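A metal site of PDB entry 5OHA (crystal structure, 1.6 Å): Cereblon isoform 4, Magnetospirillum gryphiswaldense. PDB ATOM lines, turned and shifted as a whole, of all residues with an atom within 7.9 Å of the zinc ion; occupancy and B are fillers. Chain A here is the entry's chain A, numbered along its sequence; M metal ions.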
ATOM      1  N   ARG A  24     -28.009  18.481   4.128  1.00  0.00           N
ATOM      2  CA  ARG A  24     -26.789  18.991   4.671  1.00  0.00           C
ATOM      3  C   ARG A  24     -25.585  18.568   3.829  1.00  0.00           C
ATOM      4  O   ARG A  24     -25.650  17.548   3.151  1.00  0.00           O
ATOM      5  CB  ARG A  24     -26.606  18.497   6.143  1.00  0.00           C
ATOM      6  CG  ARG A  24     -27.641  19.058   7.086  1.00  0.00           C
ATOM      7  CD  ARG A  24     -27.385  18.636   8.560  1.00  0.00           C
ATOM      8  NE  ARG A  24     -28.351  19.250   9.412  1.00  0.00           N
ATOM      9  CZ  ARG A  24     -28.303  20.504   9.826  1.00  0.00           C
ATOM     10  NH1 ARG A  24     -27.189  21.209   9.603  1.00  0.00           N
ATOM     11  NH2 ARG A  24     -29.282  21.027  10.538  1.00  0.00           N
ATOM     12  N   CYS A  25     -24.452  19.271   3.925  1.00  0.00           N
ATOM     13  CA  CYS A  25     -23.199  18.815   3.339  1.00  0.00           C
ATOM     14  C   CYS A  25     -22.821  17.461   3.927  1.00  0.00           C
ATOM     15  O   CYS A  25     -22.730  17.306   5.172  1.00  0.00           O
ATOM     16  CB  CYS A  25     -22.110  19.819   3.589  1.00  0.00           C
ATOM     17  SG  CYS A  25     -20.483  19.271   2.957  1.00  0.00           S
ATOM     18  N   ARG A  26     -22.596  16.437   3.113  1.00  0.00           N
ATOM     19  CA  ARG A  26     -22.201  15.134   3.580  1.00  0.00           C
ATOM     20  C   ARG A  26     -20.880  15.106   4.326  1.00  0.00           C
ATOM     21  O   ARG A  26     -20.650  14.206   5.154  1.00  0.00           O
ATOM     22  CB  ARG A  26     -22.174  14.176   2.347  1.00  0.00           C
ATOM     23  CG  ARG A  26     -21.723  12.835   2.583  1.00  0.00           C
ATOM     24  CD  ARG A  26     -21.778  12.042   1.310  1.00  0.00           C
ATOM     25  NE  ARG A  26     -21.239  10.769   1.573  1.00  0.00           N
ATOM     26  CZ  ARG A  26     -21.084   9.818   0.666  1.00  0.00           C
ATOM     27  NH1 ARG A  26     -21.566   9.984  -0.578  1.00  0.00           N
ATOM     28  NH2 ARG A  26     -20.500   8.704   1.010  1.00  0.00           N
ATOM     29  N   GLN A  27     -19.995  16.033   3.948  1.00  0.00           N
ATOM     30  CA  GLN A  27     -18.636  16.011   4.536  1.00  0.00           C
ATOM     31  C   GLN A  27     -18.545  16.718   5.861  1.00  0.00           C
ATOM     32  O   GLN A  27     -17.626  16.420   6.621  1.00  0.00           O
ATOM     33  CB  GLN A  27     -17.661  16.606   3.575  1.00  0.00           C
ATOM     34  CG  GLN A  27     -17.596  15.804   2.315  1.00  0.00           C
ATOM     35  CD  GLN A  27     -17.259  14.337   2.544  1.00  0.00           C
ATOM     36  OE1 GLN A  27     -17.943  13.420   2.020  1.00  0.00           O
ATOM     37  NE2 GLN A  27     -16.212  14.080   3.308  1.00  0.00           N
ATOM     38  N   CYS A  28     -19.477  17.597   6.204  1.00  0.00           N
ATOM     39  CA  CYS A  28     -19.322  18.368   7.431  1.00  0.00           C
ATOM     40  C   CYS A  28     -20.602  18.705   8.170  1.00  0.00           C
ATOM     41  O   CYS A  28     -20.578  19.160   9.328  1.00  0.00           O
ATOM     42  CB  CYS A  28     -18.557  19.655   7.162  1.00  0.00           C
ATOM     43  SG  CYS A  28     -19.536  20.924   6.295  1.00  0.00           S
ATOM     44  N   GLY A  29     -21.765  18.574   7.539  1.00  0.00           N
ATOM     45  CA  GLY A  29     -22.973  18.952   8.196  1.00  0.00           C
ATOM     46  C   GLY A  29     -23.619  20.279   7.992  1.00  0.00           C
ATOM     47  O   GLY A  29     -24.778  20.540   8.435  1.00  0.00           O
ATOM     48  N   GLN A  30     -22.918  21.163   7.264  1.00  0.00           N
ATOM     49  CA  GLN A  30     -23.452  22.444   6.983  1.00  0.00           C
ATOM     50  C   GLN A  30     -24.899  22.351   6.402  1.00  0.00           C
ATOM     51  O   GLN A  30     -25.114  21.543   5.497  1.00  0.00           O
ATOM     52  CB  GLN A  30     -22.519  23.097   5.931  1.00  0.00           C
ATOM     53  CG  GLN A  30     -22.968  24.431   5.379  1.00  0.00           C
ATOM     54  CD  GLN A  30     -22.632  25.572   6.265  1.00  0.00           C
ATOM     55  OE1 GLN A  30     -22.776  25.488   7.476  1.00  0.00           O
ATOM     56  NE2 GLN A  30     -22.201  26.677   5.679  1.00  0.00           N
ATOM     57  N   THR A  31     -25.831  23.180   6.882  1.00  0.00           N
ATOM     58  CA  THR A  31     -27.174  23.219   6.296  1.00  0.00           C
ATOM     59  C   THR A  31     -27.117  23.815   4.873  1.00  0.00           C
ATOM     60  O   THR A  31     -26.549  24.891   4.703  1.00  0.00           O
ATOM     61  CB  THR A  31     -28.120  24.049   7.155  1.00  0.00           C
ATOM     62  OG1 THR A  31     -28.048  23.657   8.535  1.00  0.00           O
ATOM     63  CG2 THR A  31     -29.467  23.834   6.723  1.00  0.00           C
ATOM     64  N   ILE A  32     -27.676  23.120   3.871  1.00  0.00           N
ATOM     65  CA  ILE A  32     -27.590  23.530   2.462  1.00  0.00           C
ATOM     66  C   ILE A  32     -28.961  23.779   1.793  1.00  0.00           C
ATOM     67  O   ILE A  32     -29.176  24.852   1.229  1.00  0.00           O
ATOM     68  CB  ILE A  32     -26.768  22.552   1.593  1.00  0.00           C
ATOM     69  CG1 ILE A  32     -25.364  22.301   2.121  1.00  0.00           C
ATOM     70  CG2 ILE A  32     -26.771  23.077   0.151  1.00  0.00           C
ATOM     71  CD1 ILE A  32     -24.473  23.509   2.159  1.00  0.00           C
ATOM     72  N   GLY A  67     -25.752  28.387   2.809  1.00  0.00           N
ATOM     73  CA  GLY A  67     -24.508  27.782   3.332  1.00  0.00           C
ATOM     74  C   GLY A  67     -23.418  27.424   2.343  1.00  0.00           C
ATOM     75  O   GLY A  67     -22.496  26.671   2.674  1.00  0.00           O
ATOM     76  N   LEU A  90     -19.305  25.918  -3.590  1.00  0.00           N
ATOM     77  CA  LEU A  90     -18.619  25.111  -2.564  1.00  0.00           C
ATOM     78  C   LEU A  90     -19.488  25.150  -1.283  1.00  0.00           C
ATOM     79  O   LEU A  90     -20.170  26.146  -1.020  1.00  0.00           O
ATOM     80  CB  LEU A  90     -17.234  25.630  -2.308  1.00  0.00           C
ATOM     81  CG  LEU A  90     -16.264  25.736  -3.508  1.00  0.00           C
ATOM     82  CD1 LEU A  90     -14.956  26.231  -2.942  1.00  0.00           C
ATOM     83  CD2 LEU A  90     -16.196  24.404  -4.246  1.00  0.00           C
ATOM     84  N   CYS A  91     -19.378  24.096  -0.501  1.00  0.00           N
ATOM     85  CA  CYS A  91     -19.852  24.182   0.890  1.00  0.00           C
ATOM     86  C   CYS A  91     -19.087  25.361   1.510  1.00  0.00           C
ATOM     87  O   CYS A  91     -17.853  25.448   1.493  1.00  0.00           O
ATOM     88  CB  CYS A  91     -19.570  22.908   1.635  1.00  0.00           C
ATOM     89  SG  CYS A  91     -19.995  23.029   3.384  1.00  0.00           S
ATOM     90  N   GLY A  92     -19.845  26.305   2.093  1.00  0.00           N
ATOM     91  CA  GLY A  92     -19.279  27.453   2.747  1.00  0.00           C
ATOM     92  C   GLY A  92     -18.469  27.190   3.974  1.00  0.00           C
ATOM     93  O   GLY A  92     -17.654  28.012   4.392  1.00  0.00           O
ATOM     94  N   GLN A  93     -18.674  26.014   4.543  1.00  0.00           N
ATOM     95  CA  GLN A  93     -17.999  25.623   5.732  1.00  0.00           C
ATOM     96  C   GLN A  93     -16.724  24.850   5.418  1.00  0.00           C
ATOM     97  O   GLN A  93     -15.655  25.278   5.813  1.00  0.00           O
ATOM     98  CB  GLN A  93     -18.951  24.800   6.661  1.00  0.00           C
ATOM     99  CG  GLN A  93     -18.430  24.348   8.001  1.00  0.00           C
ATOM    100  CD  GLN A  93     -19.527  24.036   9.000  1.00  0.00           C
ATOM    101  OE1 GLN A  93     -19.863  24.868   9.799  1.00  0.00           O
ATOM    102  NE2 GLN A  93     -20.068  22.824   8.927  1.00  0.00           N
ATOM    103  N   CYS A  94     -16.832  23.711   4.691  1.00  0.00           N
ATOM    104  CA  CYS A  94     -15.694  22.845   4.483  1.00  0.00           C
ATOM    105  C   CYS A  94     -15.028  22.933   3.102  1.00  0.00           C
ATOM    106  O   CYS A  94     -13.932  22.383   2.951  1.00  0.00           O
ATOM    107  CB  CYS A  94     -16.051  21.407   4.770  1.00  0.00           C
ATOM    108  SG  CYS A  94     -16.959  20.544   3.453  1.00  0.00           S
ATOM    109  N   GLY A  95     -15.645  23.612   2.153  1.00  0.00           N
ATOM    110  CA  GLY A  95     -15.027  23.744   0.824  1.00  0.00           C
ATOM    111  C   GLY A  95     -15.330  22.636  -0.163  1.00  0.00           C
ATOM    112  O   GLY A  95     -14.878  22.719  -1.317  1.00  0.00           O
ATOM    113  N   SER A  96     -16.092  21.642   0.248  1.00  0.00           N
ATOM    114  CA  SER A  96     -16.493  20.537  -0.654  1.00  0.00           C
ATOM    115  C   SER A  96     -17.262  21.077  -1.849  1.00  0.00           C
ATOM    116  O   SER A  96     -18.109  21.959  -1.721  1.00  0.00           O
ATOM    117  CB  SER A  96     -17.414  19.576   0.090  1.00  0.00           C
ATOM    118  OG  SER A  96     -17.870  18.475  -0.724  1.00  0.00           O
ATOM    119  N   HIS A  97     -16.934  20.564  -3.043  1.00  0.00           N
ATOM    120  CA  HIS A  97     -17.717  21.015  -4.216  1.00  0.00           C
ATOM    121  C   HIS A  97     -19.102  20.406  -4.248  1.00  0.00           C
ATOM    122  O   HIS A  97     -19.225  19.196  -4.411  1.00  0.00           O
ATOM    123  CB  HIS A  97     -16.959  20.672  -5.508  1.00  0.00           C
ATOM    124  CG  HIS A  97     -17.720  21.051  -6.708  1.00  0.00           C
ATOM    125  ND1 HIS A  97     -17.533  20.402  -7.923  1.00  0.00           N
ATOM    126  CD2 HIS A  97     -18.603  22.050  -6.930  1.00  0.00           C
ATOM    127  CE1 HIS A  97     -18.327  20.956  -8.818  1.00  0.00           C
ATOM    128  NE2 HIS A  97     -18.978  21.952  -8.254  1.00  0.00           N
ATOM    129  N   LEU A  98     -20.136  21.209  -3.965  1.00  0.00           N
ATOM    130  CA  LEU A  98     -21.483  20.728  -3.853  1.00  0.00           C
ATOM    131  C   LEU A  98     -22.308  20.870  -5.120  1.00  0.00           C
ATOM    132  O   LEU A  98     -23.321  20.223  -5.277  1.00  0.00           O
ATOM    133  CB  LEU A  98     -22.221  21.376  -2.674  1.00  0.00           C
ATOM    134  CG  LEU A  98     -21.619  20.999  -1.306  1.00  0.00           C
ATOM    135  CD1 LEU A  98     -22.508  21.536  -0.186  1.00  0.00           C
ATOM    136  CD2 LEU A  98     -21.324  19.552  -1.105  1.00  0.00           C
ATOM    137  N   ARG A 118     -23.421  14.290  -2.780  1.00  0.00           N
ATOM    138  CA  ARG A 118     -22.572  15.032  -1.891  1.00  0.00           C
ATOM    139  C   ARG A 118     -23.400  15.652  -0.744  1.00  0.00           C
ATOM    140  O   ARG A 118     -22.877  16.440   0.058  1.00  0.00           O
ATOM    141  CB  ARG A 118     -21.707  16.004  -2.695  1.00  0.00           C
ATOM    142  CG  ARG A 118     -20.886  15.292  -3.749  1.00  0.00           C
ATOM    143  CD  ARG A 118     -19.884  16.207  -4.407  1.00  0.00           C
ATOM    144  NE  ARG A 118     -19.312  15.467  -5.501  1.00  0.00           N
ATOM    145  CZ  ARG A 118     -18.402  15.948  -6.307  1.00  0.00           C
ATOM    146  NH1 ARG A 118     -17.948  17.181  -6.103  1.00  0.00           N
ATOM    147  NH2 ARG A 118     -17.984  15.198  -7.306  1.00  0.00           N
HETATM  148 ZN    ZN M   1     -19.207  20.857   4.028  1.00  0.00          ZN
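The zinc ion is bound by SG of Cys 28 (2.3 Å), SG of Cys 25 (2.3 Å), SG of Cys 94 (2.3 Å) and SG of Cys 91 (2.4 Å).
Four residues have an atom within 4 Å of the zinc ion: Cys 25, Cys 28, Cys 91 and Cys 94. The nearest printed residue that does not touch the zinc ion is Gln 30 (4.4 Å).
SG of Cys 28 lies close to N of Gln 30, 3.5 Å away. SG of Cys 28 lies close to NE2 of Gln 93 (3.3 Å). The side-chain sulfur (SG) of Cys 25 sits close to the backbone NH (N) of Gln 27 (3.4 Å). The side-chain sulfur (SG) of Cys 94 sits close to the backbone NH (N) of Ser 96 (3.5 Å). O of Ser 96 sits at hydrogen-bond distance from N of Cys 91, 2.8 Å away. O of Gln 30 is in hydrogen-bond range of N of Cys 25 (2.8 Å). The backbone NH of Gln 93 lies close to the side-chain sulfur of Cys 91 (3.5 Å).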
